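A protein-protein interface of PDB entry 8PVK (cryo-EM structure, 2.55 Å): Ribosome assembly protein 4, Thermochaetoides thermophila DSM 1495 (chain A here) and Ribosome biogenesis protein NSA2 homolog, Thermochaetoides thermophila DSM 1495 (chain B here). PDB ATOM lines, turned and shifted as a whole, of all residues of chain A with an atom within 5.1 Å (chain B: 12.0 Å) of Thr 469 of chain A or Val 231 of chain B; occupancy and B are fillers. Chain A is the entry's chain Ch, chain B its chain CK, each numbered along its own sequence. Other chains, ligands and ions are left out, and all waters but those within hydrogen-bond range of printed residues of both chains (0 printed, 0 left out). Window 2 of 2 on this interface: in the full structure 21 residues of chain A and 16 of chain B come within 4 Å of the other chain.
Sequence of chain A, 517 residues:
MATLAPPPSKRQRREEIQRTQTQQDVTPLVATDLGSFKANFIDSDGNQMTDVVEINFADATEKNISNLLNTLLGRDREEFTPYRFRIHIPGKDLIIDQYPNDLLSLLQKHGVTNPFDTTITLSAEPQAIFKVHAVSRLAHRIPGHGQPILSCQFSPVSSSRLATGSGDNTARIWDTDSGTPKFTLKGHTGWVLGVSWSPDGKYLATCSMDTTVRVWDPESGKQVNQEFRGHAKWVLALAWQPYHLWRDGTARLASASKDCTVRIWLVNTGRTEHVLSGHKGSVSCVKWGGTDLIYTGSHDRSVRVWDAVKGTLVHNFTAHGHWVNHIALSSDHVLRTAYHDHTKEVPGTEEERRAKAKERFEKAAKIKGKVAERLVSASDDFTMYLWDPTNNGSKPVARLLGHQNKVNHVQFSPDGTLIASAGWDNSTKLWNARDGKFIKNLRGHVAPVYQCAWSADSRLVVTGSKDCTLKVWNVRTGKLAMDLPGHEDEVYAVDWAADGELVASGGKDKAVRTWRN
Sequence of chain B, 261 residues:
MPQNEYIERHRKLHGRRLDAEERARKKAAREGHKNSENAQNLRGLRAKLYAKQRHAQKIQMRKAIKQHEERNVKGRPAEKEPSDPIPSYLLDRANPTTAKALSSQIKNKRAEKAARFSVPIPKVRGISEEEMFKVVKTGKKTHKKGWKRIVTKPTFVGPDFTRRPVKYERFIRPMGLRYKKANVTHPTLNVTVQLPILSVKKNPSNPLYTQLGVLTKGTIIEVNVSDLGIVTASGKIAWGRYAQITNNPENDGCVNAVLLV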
ATOM      1  N   HIS A 445      21.606   4.245  -8.980  1.00  0.00           N
ATOM      2  CA  HIS A 445      22.111   4.764 -10.243  1.00  0.00           C
ATOM      3  C   HIS A 445      22.532   3.615 -11.153  1.00  0.00           C
ATOM      4  O   HIS A 445      23.019   2.579 -10.694  1.00  0.00           O
ATOM      5  CB  HIS A 445      23.291   5.710 -10.015  1.00  0.00           C
ATOM      6  CG  HIS A 445      22.887   7.113  -9.687  1.00  0.00           C
ATOM      7  ND1 HIS A 445      22.074   7.864 -10.508  1.00  0.00           N
ATOM      8  CD2 HIS A 445      23.194   7.907  -8.634  1.00  0.00           C
ATOM      9  CE1 HIS A 445      21.893   9.058  -9.972  1.00  0.00           C
ATOM     10  NE2 HIS A 445      22.562   9.110  -8.835  1.00  0.00           N
ATOM     11  N   VAL A 446      22.334   3.808 -12.455  1.00  0.00           N
ATOM     12  CA  VAL A 446      22.603   2.778 -13.450  1.00  0.00           C
ATOM     13  C   VAL A 446      23.741   3.148 -14.386  1.00  0.00           C
ATOM     14  O   VAL A 446      24.098   2.350 -15.258  1.00  0.00           O
ATOM     15  CB  VAL A 446      21.334   2.437 -14.257  1.00  0.00           C
ATOM     16  CG1 VAL A 446      20.352   1.670 -13.392  1.00  0.00           C
ATOM     17  CG2 VAL A 446      20.689   3.698 -14.786  1.00  0.00           C
ATOM     18  N   THR A 463      23.144  13.308  -5.676  1.00  0.00           N
ATOM     19  CA  THR A 463      24.135  12.743  -6.580  1.00  0.00           C
ATOM     20  C   THR A 463      23.647  12.900  -8.009  1.00  0.00           C
ATOM     21  O   THR A 463      22.533  12.486  -8.337  1.00  0.00           O
ATOM     22  CB  THR A 463      24.396  11.268  -6.270  1.00  0.00           C
ATOM     23  OG1 THR A 463      23.162  10.541  -6.321  1.00  0.00           O
ATOM     24  CG2 THR A 463      25.009  11.116  -4.888  1.00  0.00           C
ATOM     25  N   GLY A 464      24.486  13.494  -8.851  1.00  0.00           N
ATOM     26  CA  GLY A 464      24.209  13.633 -10.268  1.00  0.00           C
ATOM     27  C   GLY A 464      25.089  12.680 -11.057  1.00  0.00           C
ATOM     28  O   GLY A 464      26.312  12.647 -10.867  1.00  0.00           O
ATOM     29  N   SER A 465      24.453  11.909 -11.941  1.00  0.00           N
ATOM     30  CA  SER A 465      25.161  10.807 -12.578  1.00  0.00           C
ATOM     31  C   SER A 465      25.084  10.911 -14.096  1.00  0.00           C
ATOM     32  O   SER A 465      24.447  11.804 -14.660  1.00  0.00           O
ATOM     33  CB  SER A 465      24.616   9.456 -12.104  1.00  0.00           C
ATOM     34  OG  SER A 465      25.100   8.400 -12.915  1.00  0.00           O
ATOM     35  N   ASP A 467      23.581   8.789 -15.897  1.00  0.00           N
ATOM     36  CA  ASP A 467      22.282   8.273 -16.314  1.00  0.00           C
ATOM     37  C   ASP A 467      21.209   9.350 -16.413  1.00  0.00           C
ATOM     38  O   ASP A 467      20.026   9.017 -16.263  1.00  0.00           O
ATOM     39  CB  ASP A 467      21.821   7.149 -15.376  1.00  0.00           C
ATOM     40  CG  ASP A 467      21.647   7.592 -13.925  1.00  0.00           C
ATOM     41  OD1 ASP A 467      21.845   8.778 -13.594  1.00  0.00           O
ATOM     42  OD2 ASP A 467      21.303   6.724 -13.098  1.00  0.00           O
ATOM     43  N   CYS A 468      21.618  10.612 -16.578  1.00  0.00           N
ATOM     44  CA  CYS A 468      20.767  11.765 -16.862  1.00  0.00           C
ATOM     45  C   CYS A 468      19.934  12.189 -15.659  1.00  0.00           C
ATOM     46  O   CYS A 468      18.996  12.977 -15.808  1.00  0.00           O
ATOM     47  CB  CYS A 468      19.845  11.504 -18.062  1.00  0.00           C
ATOM     48  SG  CYS A 468      20.696  11.139 -19.604  1.00  0.00           S
ATOM     49  N   THR A 469      20.240  11.684 -14.465  1.00  0.00           N
ATOM     50  CA  THR A 469      19.393  11.905 -13.301  1.00  0.00           C
ATOM     51  C   THR A 469      20.188  12.423 -12.109  1.00  0.00           C
ATOM     52  O   THR A 469      21.405  12.205 -11.975  1.00  0.00           O
ATOM     53  CB  THR A 469      18.646  10.627 -12.862  1.00  0.00           C
ATOM     54  OG1 THR A 469      19.576   9.681 -12.322  1.00  0.00           O
ATOM     55  CG2 THR A 469      17.863  10.000 -14.006  1.00  0.00           C
ATOM     56  N   LEU A 470      19.447  13.103 -11.233  1.00  0.00           N
ATOM     57  CA  LEU A 470      19.872  13.428  -9.882  1.00  0.00           C
ATOM     58  C   LEU A 470      19.083  12.559  -8.913  1.00  0.00           C
ATOM     59  O   LEU A 470      17.918  12.239  -9.160  1.00  0.00           O
ATOM     60  CB  LEU A 470      19.624  14.900  -9.545  1.00  0.00           C
ATOM     61  CG  LEU A 470      20.066  16.057 -10.443  1.00  0.00           C
ATOM     62  CD1 LEU A 470      20.060  17.335  -9.629  1.00  0.00           C
ATOM     63  CD2 LEU A 470      21.424  15.831 -11.063  1.00  0.00           C
ATOM     64  N   LYS A 471      19.717  12.160  -7.819  1.00  0.00           N
ATOM     65  CA  LYS A 471      19.033  11.406  -6.778  1.00  0.00           C
ATOM     66  C   LYS A 471      19.364  12.001  -5.421  1.00  0.00           C
ATOM     67  O   LYS A 471      20.538  12.199  -5.096  1.00  0.00           O
ATOM     68  CB  LYS A 471      19.405   9.922  -6.815  1.00  0.00           C
ATOM     69  CG  LYS A 471      18.984   9.214  -8.089  1.00  0.00           C
ATOM     70  CD  LYS A 471      18.844   7.721  -7.887  1.00  0.00           C
ATOM     71  CE  LYS A 471      18.872   6.994  -9.217  1.00  0.00           C
ATOM     72  NZ  LYS A 471      18.032   7.677 -10.236  1.00  0.00           N
ATOM     73  N   ASP A 483      13.820  11.352  -6.420  1.00  0.00           N
ATOM     74  CA  ASP A 483      14.387  11.125  -7.742  1.00  0.00           C
ATOM     75  C   ASP A 483      14.092  12.332  -8.620  1.00  0.00           C
ATOM     76  O   ASP A 483      12.961  12.825  -8.645  1.00  0.00           O
ATOM     77  CB  ASP A 483      13.812   9.857  -8.378  1.00  0.00           C
ATOM     78  CG  ASP A 483      14.749   9.235  -9.392  1.00  0.00           C
ATOM     79  OD1 ASP A 483      15.690   9.923  -9.839  1.00  0.00           O
ATOM     80  OD2 ASP A 483      14.542   8.056  -9.746  1.00  0.00           O
ATOM     81  N   LEU A 484      15.106  12.807  -9.345  1.00  0.00           N
ATOM     82  CA  LEU A 484      14.996  14.006 -10.172  1.00  0.00           C
ATOM     83  C   LEU A 484      15.443  13.668 -11.587  1.00  0.00           C
ATOM     84  O   LEU A 484      16.640  13.737 -11.907  1.00  0.00           O
ATOM     85  CB  LEU A 484      15.824  15.151  -9.592  1.00  0.00           C
ATOM     86  CG  LEU A 484      15.566  15.523  -8.130  1.00  0.00           C
ATOM     87  CD1 LEU A 484      16.552  16.577  -7.662  1.00  0.00           C
ATOM     88  CD2 LEU A 484      14.137  16.000  -7.939  1.00  0.00           C
ATOM     89  N   PRO A 485      14.519  13.250 -12.445  1.00  0.00           N
ATOM     90  CA  PRO A 485      14.809  13.148 -13.874  1.00  0.00           C
ATOM     91  C   PRO A 485      14.473  14.455 -14.583  1.00  0.00           C
ATOM     92  O   PRO A 485      13.857  15.361 -14.020  1.00  0.00           O
ATOM     93  CB  PRO A 485      13.878  12.021 -14.331  1.00  0.00           C
ATOM     94  CG  PRO A 485      12.692  12.166 -13.443  1.00  0.00           C
ATOM     95  CD  PRO A 485      13.203  12.675 -12.113  1.00  0.00           C
ATOM     96  N   VAL A 491      24.872  14.440 -16.700  1.00  0.00           N
ATOM     97  CA  VAL A 491      24.980  15.515 -15.721  1.00  0.00           C
ATOM     98  C   VAL A 491      26.444  15.658 -15.328  1.00  0.00           C
ATOM     99  O   VAL A 491      27.081  14.686 -14.909  1.00  0.00           O
ATOM    100  CB  VAL A 491      24.102  15.241 -14.493  1.00  0.00           C
ATOM    101  CG1 VAL A 491      24.298  16.326 -13.453  1.00  0.00           C
ATOM    102  CG2 VAL A 491      22.643  15.144 -14.896  1.00  0.00           C
ATOM    103  N   TYR B  89      37.466  16.399 -14.639  1.00  0.00           N
ATOM    104  CA  TYR B  89      37.674  15.023 -14.203  1.00  0.00           C
ATOM    105  C   TYR B  89      37.516  14.018 -15.338  1.00  0.00           C
ATOM    106  O   TYR B  89      37.947  12.870 -15.194  1.00  0.00           O
ATOM    107  CB  TYR B  89      36.726  14.678 -13.052  1.00  0.00           C
ATOM    108  CG  TYR B  89      35.263  14.974 -13.306  1.00  0.00           C
ATOM    109  CD1 TYR B  89      34.445  14.050 -13.943  1.00  0.00           C
ATOM    110  CD2 TYR B  89      34.696  16.170 -12.884  1.00  0.00           C
ATOM    111  CE1 TYR B  89      33.111  14.315 -14.169  1.00  0.00           C
ATOM    112  CE2 TYR B  89      33.361  16.443 -13.105  1.00  0.00           C
ATOM    113  CZ  TYR B  89      32.574  15.512 -13.747  1.00  0.00           C
ATOM    114  OH  TYR B  89      31.244  15.776 -13.969  1.00  0.00           O
ATOM    115  N   HIS B 186      25.221   1.013 -29.505  1.00  0.00           N
ATOM    116  CA  HIS B 186      24.369   2.187 -29.393  1.00  0.00           C
ATOM    117  C   HIS B 186      24.826   3.222 -30.411  1.00  0.00           C
ATOM    118  O   HIS B 186      25.969   3.688 -30.328  1.00  0.00           O
ATOM    119  CB  HIS B 186      24.434   2.770 -27.991  1.00  0.00           C
ATOM    120  CG  HIS B 186      23.250   3.611 -27.628  1.00  0.00           C
ATOM    121  ND1 HIS B 186      22.865   4.713 -28.359  1.00  0.00           N
ATOM    122  CD2 HIS B 186      22.369   3.513 -26.604  1.00  0.00           C
ATOM    123  CE1 HIS B 186      21.797   5.256 -27.805  1.00  0.00           C
ATOM    124  NE2 HIS B 186      21.475   4.547 -26.738  1.00  0.00           N
ATOM    125  N   LEU B 189      25.477   6.794 -28.391  1.00  0.00           N
ATOM    126  CA  LEU B 189      26.552   6.758 -27.409  1.00  0.00           C
ATOM    127  C   LEU B 189      27.879   6.292 -27.990  1.00  0.00           C
ATOM    128  O   LEU B 189      28.914   6.501 -27.345  1.00  0.00           O
ATOM    129  CB  LEU B 189      26.160   5.852 -26.241  1.00  0.00           C
ATOM    130  CG  LEU B 189      24.986   6.336 -25.392  1.00  0.00           C
ATOM    131  CD1 LEU B 189      24.607   5.289 -24.358  1.00  0.00           C
ATOM    132  CD2 LEU B 189      25.327   7.654 -24.719  1.00  0.00           C
ATOM    133  N   ASN B 224      18.533  -6.999 -23.549  1.00  0.00           N
ATOM    134  CA  ASN B 224      18.613  -6.444 -22.206  1.00  0.00           C
ATOM    135  C   ASN B 224      19.616  -5.297 -22.218  1.00  0.00           C
ATOM    136  O   ASN B 224      20.796  -5.504 -22.514  1.00  0.00           O
ATOM    137  CB  ASN B 224      19.031  -7.530 -21.213  1.00  0.00           C
ATOM    138  CG  ASN B 224      18.759  -7.153 -19.765  1.00  0.00           C
ATOM    139  OD1 ASN B 224      18.669  -5.978 -19.414  1.00  0.00           O
ATOM    140  ND2 ASN B 224      18.630  -8.162 -18.916  1.00  0.00           N
ATOM    141  N   VAL B 225      19.150  -4.096 -21.882  1.00  0.00           N
ATOM    142  CA  VAL B 225      19.979  -2.899 -21.960  1.00  0.00           C
ATOM    143  C   VAL B 225      20.194  -2.321 -20.566  1.00  0.00           C
ATOM    144  O   VAL B 225      20.297  -1.102 -20.398  1.00  0.00           O
ATOM    145  CB  VAL B 225      19.358  -1.854 -22.907  1.00  0.00           C
ATOM    146  CG1 VAL B 225      19.493  -2.305 -24.349  1.00  0.00           C
ATOM    147  CG2 VAL B 225      17.896  -1.622 -22.567  1.00  0.00           C
ATOM    148  N   SER B 226      20.253  -3.197 -19.559  1.00  0.00           N
ATOM    149  CA  SER B 226      20.513  -2.750 -18.194  1.00  0.00           C
ATOM    150  C   SER B 226      21.911  -2.163 -18.045  1.00  0.00           C
ATOM    151  O   SER B 226      22.104  -1.209 -17.283  1.00  0.00           O
ATOM    152  CB  SER B 226      20.332  -3.908 -17.215  1.00  0.00           C
ATOM    153  OG  SER B 226      18.983  -4.325 -17.150  1.00  0.00           O
ATOM    154  N   ASP B 227      22.896  -2.719 -18.756  1.00  0.00           N
ATOM    155  CA  ASP B 227      24.265  -2.229 -18.651  1.00  0.00           C
ATOM    156  C   ASP B 227      24.466  -0.896 -19.357  1.00  0.00           C
ATOM    157  O   ASP B 227      25.497  -0.249 -19.146  1.00  0.00           O
ATOM    158  CB  ASP B 227      25.237  -3.264 -19.216  1.00  0.00           C
ATOM    159  CG  ASP B 227      25.423  -4.452 -18.296  1.00  0.00           C
ATOM    160  OD1 ASP B 227      25.001  -4.367 -17.124  1.00  0.00           O
ATOM    161  OD2 ASP B 227      25.991  -5.469 -18.743  1.00  0.00           O
ATOM    162  N   LEU B 228      23.516  -0.473 -20.189  1.00  0.00           N
ATOM    163  CA  LEU B 228      23.648   0.783 -20.912  1.00  0.00           C
ATOM    164  C   LEU B 228      23.138   1.983 -20.129  1.00  0.00           C
ATOM    165  O   LEU B 228      23.366   3.119 -20.559  1.00  0.00           O
ATOM    166  CB  LEU B 228      22.920   0.686 -22.252  1.00  0.00           C
ATOM    167  CG  LEU B 228      23.687  -0.117 -23.301  1.00  0.00           C
ATOM    168  CD1 LEU B 228      22.802  -0.436 -24.482  1.00  0.00           C
ATOM    169  CD2 LEU B 228      24.922   0.649 -23.749  1.00  0.00           C
ATOM    170  N   GLY B 229      22.469   1.764 -18.998  1.00  0.00           N
ATOM    171  CA  GLY B 229      22.032   2.845 -18.135  1.00  0.00           C
ATOM    172  C   GLY B 229      21.008   3.785 -18.738  1.00  0.00           C
ATOM    173  O   GLY B 229      21.148   5.007 -18.633  1.00  0.00           O
ATOM    174  N   ILE B 230      19.979   3.235 -19.370  1.00  0.00           N
ATOM    175  CA  ILE B 230      18.939   4.036 -20.007  1.00  0.00           C
ATOM    176  C   ILE B 230      17.831   4.302 -18.997  1.00  0.00           C
ATOM    177  O   ILE B 230      17.289   3.369 -18.393  1.00  0.00           O
ATOM    178  CB  ILE B 230      18.391   3.330 -21.257  1.00  0.00           C
ATOM    179  CG1 ILE B 230      19.512   3.109 -22.274  1.00  0.00           C
ATOM    180  CG2 ILE B 230      17.258   4.134 -21.872  1.00  0.00           C
ATOM    181  CD1 ILE B 230      19.075   2.371 -23.516  1.00  0.00           C
ATOM    182  N   VAL B 231      17.499   5.577 -18.808  1.00  0.00           N
ATOM    183  CA  VAL B 231      16.450   6.004 -17.891  1.00  0.00           C
ATOM    184  C   VAL B 231      15.380   6.724 -18.698  1.00  0.00           C
ATOM    185  O   VAL B 231      15.696   7.583 -19.528  1.00  0.00           O
ATOM    186  CB  VAL B 231      16.999   6.914 -16.776  1.00  0.00           C
ATOM    187  CG1 VAL B 231      15.924   7.199 -15.739  1.00  0.00           C
ATOM    188  CG2 VAL B 231      18.211   6.278 -16.120  1.00  0.00           C
ATOM    189  N   THR B 232      14.121   6.369 -18.458  1.00  0.00           N
ATOM    190  CA  THR B 232      13.008   6.993 -19.154  1.00  0.00           C
ATOM    191  C   THR B 232      12.753   8.399 -18.613  1.00  0.00           C
ATOM    192  O   THR B 232      13.362   8.842 -17.635  1.00  0.00           O
ATOM    193  CB  THR B 232      11.747   6.141 -19.026  1.00  0.00           C
ATOM    194  OG1 THR B 232      11.205   6.281 -17.707  1.00  0.00           O
ATOM    195  CG2 THR B 232      12.068   4.678 -19.282  1.00  0.00           C
ATOM    196  N   ALA B 233      11.834   9.107 -19.275  1.00  0.00           N
ATOM    197  CA  ALA B 233      11.525  10.482 -18.891  1.00  0.00           C
ATOM    198  C   ALA B 233      10.826  10.556 -17.539  1.00  0.00           C
ATOM    199  O   ALA B 233      10.932  11.573 -16.845  1.00  0.00           O
ATOM    200  CB  ALA B 233      10.667  11.147 -19.966  1.00  0.00           C
ATOM    201  N   SER B 234      10.113   9.502 -17.150  1.00  0.00           N
ATOM    202  CA  SER B 234       9.426   9.459 -15.868  1.00  0.00           C
ATOM    203  C   SER B 234      10.314   8.968 -14.734  1.00  0.00           C
ATOM    204  O   SER B 234       9.864   8.934 -13.584  1.00  0.00           O
ATOM    205  CB  SER B 234       8.183   8.570 -15.968  1.00  0.00           C
ATOM    206  OG  SER B 234       8.490   7.336 -16.590  1.00  0.00           O
ATOM    207  N   GLY B 235      11.556   8.588 -15.024  1.00  0.00           N
ATOM    208  CA  GLY B 235      12.471   8.104 -14.014  1.00  0.00           C
ATOM    209  C   GLY B 235      12.600   6.600 -13.924  1.00  0.00           C
ATOM    210  O   GLY B 235      13.366   6.112 -13.085  1.00  0.00           O
ATOM    211  N   LYS B 236      11.880   5.851 -14.752  1.00  0.00           N
ATOM    212  CA  LYS B 236      11.983   4.402 -14.735  1.00  0.00           C
ATOM    213  C   LYS B 236      13.210   3.945 -15.517  1.00  0.00           C
ATOM    214  O   LYS B 236      13.751   4.667 -16.357  1.00  0.00           O
ATOM    215  CB  LYS B 236      10.719   3.768 -15.316  1.00  0.00           C
ATOM    216  CG  LYS B 236       9.452   4.125 -14.563  1.00  0.00           C
ATOM    217  CD  LYS B 236       8.257   3.368 -15.109  1.00  0.00           C
ATOM    218  CE  LYS B 236       6.970   3.833 -14.451  1.00  0.00           C
ATOM    219  NZ  LYS B 236       6.954   3.528 -12.995  1.00  0.00           N
ATOM    220  N   ILE B 237      13.648   2.723 -15.228  1.00  0.00           N
ATOM    221  CA  ILE B 237      14.819   2.136 -15.868  1.00  0.00           C
ATOM    222  C   ILE B 237      14.342   1.249 -17.009  1.00  0.00           C
ATOM    223  O   ILE B 237      13.626   0.266 -16.785  1.00  0.00           O
ATOM    224  CB  ILE B 237      15.666   1.337 -14.867  1.00  0.00           C
ATOM    225  CG1 ILE B 237      16.076   2.217 -13.685  1.00  0.00           C
ATOM    226  CG2 ILE B 237      16.894   0.761 -15.552  1.00  0.00           C
ATOM    227  CD1 ILE B 237      16.817   3.469 -14.085  1.00  0.00           C
ATOM    228  N   ALA B 238      14.740   1.593 -18.229  1.00  0.00           N
ATOM    229  CA  ALA B 238      14.410   0.801 -19.409  1.00  0.00           C
ATOM    230  C   ALA B 238      15.464  -0.288 -19.566  1.00  0.00           C
ATOM    231  O   ALA B 238      16.612  -0.003 -19.921  1.00  0.00           O
ATOM    232  CB  ALA B 238      14.340   1.684 -20.650  1.00  0.00           C
ATOM    233  N   TRP B 239      15.079  -1.534 -19.298  1.00  0.00           N
ATOM    234  CA  TRP B 239      16.003  -2.654 -19.369  1.00  0.00           C
ATOM    235  C   TRP B 239      15.722  -3.593 -20.532  1.00  0.00           C
ATOM    236  O   TRP B 239      16.377  -4.632 -20.641  1.00  0.00           O
ATOM    237  CB  TRP B 239      15.989  -3.441 -18.052  1.00  0.00           C
ATOM    238  CG  TRP B 239      14.704  -4.144 -17.752  1.00  0.00           C
ATOM    239  CD1 TRP B 239      13.571  -3.595 -17.233  1.00  0.00           C
ATOM    240  CD2 TRP B 239      14.429  -5.539 -17.927  1.00  0.00           C
ATOM    241  NE1 TRP B 239      12.603  -4.557 -17.084  1.00  0.00           N
ATOM    242  CE2 TRP B 239      13.105  -5.761 -17.502  1.00  0.00           C
ATOM    243  CE3 TRP B 239      15.174  -6.621 -18.405  1.00  0.00           C
ATOM    244  CZ2 TRP B 239      12.510  -7.018 -17.541  1.00  0.00           C
ATOM    245  CZ3 TRP B 239      14.580  -7.868 -18.445  1.00  0.00           C
ATOM    246  CH2 TRP B 239      13.262  -8.057 -18.015  1.00  0.00           C
ATOM    247  N   GLY B 240      14.770  -3.263 -21.399  1.00  0.00           N
ATOM    248  CA  GLY B 240      14.527  -4.060 -22.585  1.00  0.00           C
ATOM    249  C   GLY B 240      14.255  -3.200 -23.798  1.00  0.00           C
ATOM    250  O   GLY B 240      13.347  -2.365 -23.773  1.00  0.00           O
ATOM    251  N   ARG B 241      15.028  -3.383 -24.868  1.00  0.00           N
ATOM    252  CA  ARG B 241      14.867  -2.562 -26.062  1.00  0.00           C
ATOM    253  C   ARG B 241      14.984  -3.437 -27.301  1.00  0.00           C
ATOM    254  O   ARG B 241      15.187  -4.650 -27.215  1.00  0.00           O
ATOM    255  CB  ARG B 241      15.886  -1.417 -26.093  1.00  0.00           C
ATOM    256  CG  ARG B 241      15.432  -0.178 -25.345  1.00  0.00           C
ATOM    257  CD  ARG B 241      16.275   1.028 -25.708  1.00  0.00           C
ATOM    258  NE  ARG B 241      15.893   1.587 -26.998  1.00  0.00           N
ATOM    259  CZ  ARG B 241      14.999   2.553 -27.158  1.00  0.00           C
ATOM    260  NH1 ARG B 241      14.371   3.092 -26.127  1.00  0.00           N
ATOM    261  NH2 ARG B 241      14.728   2.989 -28.384  1.00  0.00           N
ATOM    262  N   LEU B 259      21.214  -0.974 -31.874  1.00  0.00           N
ATOM    263  CA  LEU B 259      19.987  -0.556 -31.205  1.00  0.00           C
ATOM    264  C   LEU B 259      19.143   0.337 -32.104  1.00  0.00           C
ATOM    265  O   LEU B 259      19.667   1.167 -32.851  1.00  0.00           O
ATOM    266  CB  LEU B 259      20.295   0.195 -29.912  1.00  0.00           C
ATOM    267  CG  LEU B 259      20.678  -0.592 -28.668  1.00  0.00           C
ATOM    268  CD1 LEU B 259      20.949   0.377 -27.543  1.00  0.00           C
ATOM    269  CD2 LEU B 259      19.579  -1.567 -28.287  1.00  0.00           C
ATOM    270  N   VAL B 261      17.327   3.211 -31.894  1.00  0.00           N
ATOM    271  CA  VAL B 261      17.050   4.415 -31.123  1.00  0.00           C
ATOM    272  C   VAL B 261      16.938   5.612 -32.058  1.00  0.00           C
ATOM    273  O   VAL B 261      17.410   5.574 -33.195  1.00  0.00           O
ATOM    274  CB  VAL B 261      18.128   4.662 -30.054  1.00  0.00           C
ATOM    275  CG1 VAL B 261      18.110   3.554 -29.011  1.00  0.00           C
ATOM    276  CG2 VAL B 261      19.497   4.776 -30.697  1.00  0.00           C
ATOM    277  OXT VAL B 261      16.374   6.646 -31.701  1.00  0.00           O
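ND1 of His 445 of chain A lies within hydrogen-bond range of OD2 of Asp 467 of chain A. N of Val 446 of chain A sits at hydrogen-bond distance from OD2 of Asp 467 of chain A (3.2 Å). OG of Ser 465 of chain A sits close to OD1 of Asp 467 of chain A. The side-chain carboxylate of Asp 467 of chain A sits at hydrogen-bond distance from the side-chain hydroxyl of Thr 469 of chain A (2.8 Å). The side-chain hydroxyl (OG1) of Thr 469 of chain A is in hydrogen-bond range of the side-chain amino group (NZ) of Lys 471 of chain A (3.3 Å).
Among the printed residues, pairs that only touch across the chains: Asp 467 of chain A with Val 231 of chain B, Val 446 of chain A with Gly 229 of chain B, Val 446 of chain A with Val 231 of chain B, Thr 469 of chain A with Val 231 of chain B, Pro 485 of chain A with Ala 233 of chain B, Val 446 of chain A with Ile 237 of chain B and Asp 467 of chain A with Gly 229 of chain B.
Of the 23 printed residues of chain B, 4 touch a printed residue of chain A. Hydrophobic or aromatic side chains of chain B within 4 Å of the printed part of chain A: Val 231 and Ile 237. Along chain B the printed residues that touch a printed residue of chain A span positions 229 to 237. Of the 14 printed residues of chain A, 4 touch a printed residue of chain B. Printed residues of chain A that touch a printed residue of chain B: Val 446, Asp 467, Thr 469 and Pro 485. Hydrophobic or aromatic side chains of chain A that line the printed part of chain B: Val 446 and Pro 485.
Thr 469 of chain A touches just one residue of chain B: Val 231 (3.8 Å). Of chain B, only Gly 229, Val 231 and Ile 237 come within 4 Å of Val 446 of chain A. No residue of chain B comes within 4 Å of Ser 465 of chain A. Pro 485 of chain A touches one residue of chain B. Val 491 of chain A touches none of the printed residues of chain B. Printed residues of chain A within 4 Å of Ala 233 of chain B: Pro 485 (3.9 Å). Of the printed residues of chain A, Gly 229 of chain B touches Val 446 and Asp 467. Printed residues of chain A within 4 Å of Ile 237 of chain B: Val 446. The nearest residue of chain B that does not touch Thr 469 of chain A is Gly 235 of chain B (5.7 Å). The nearest printed residue of chain A that does not touch Val 231 of chain B is Pro 485 of chain A (5.4 Å).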
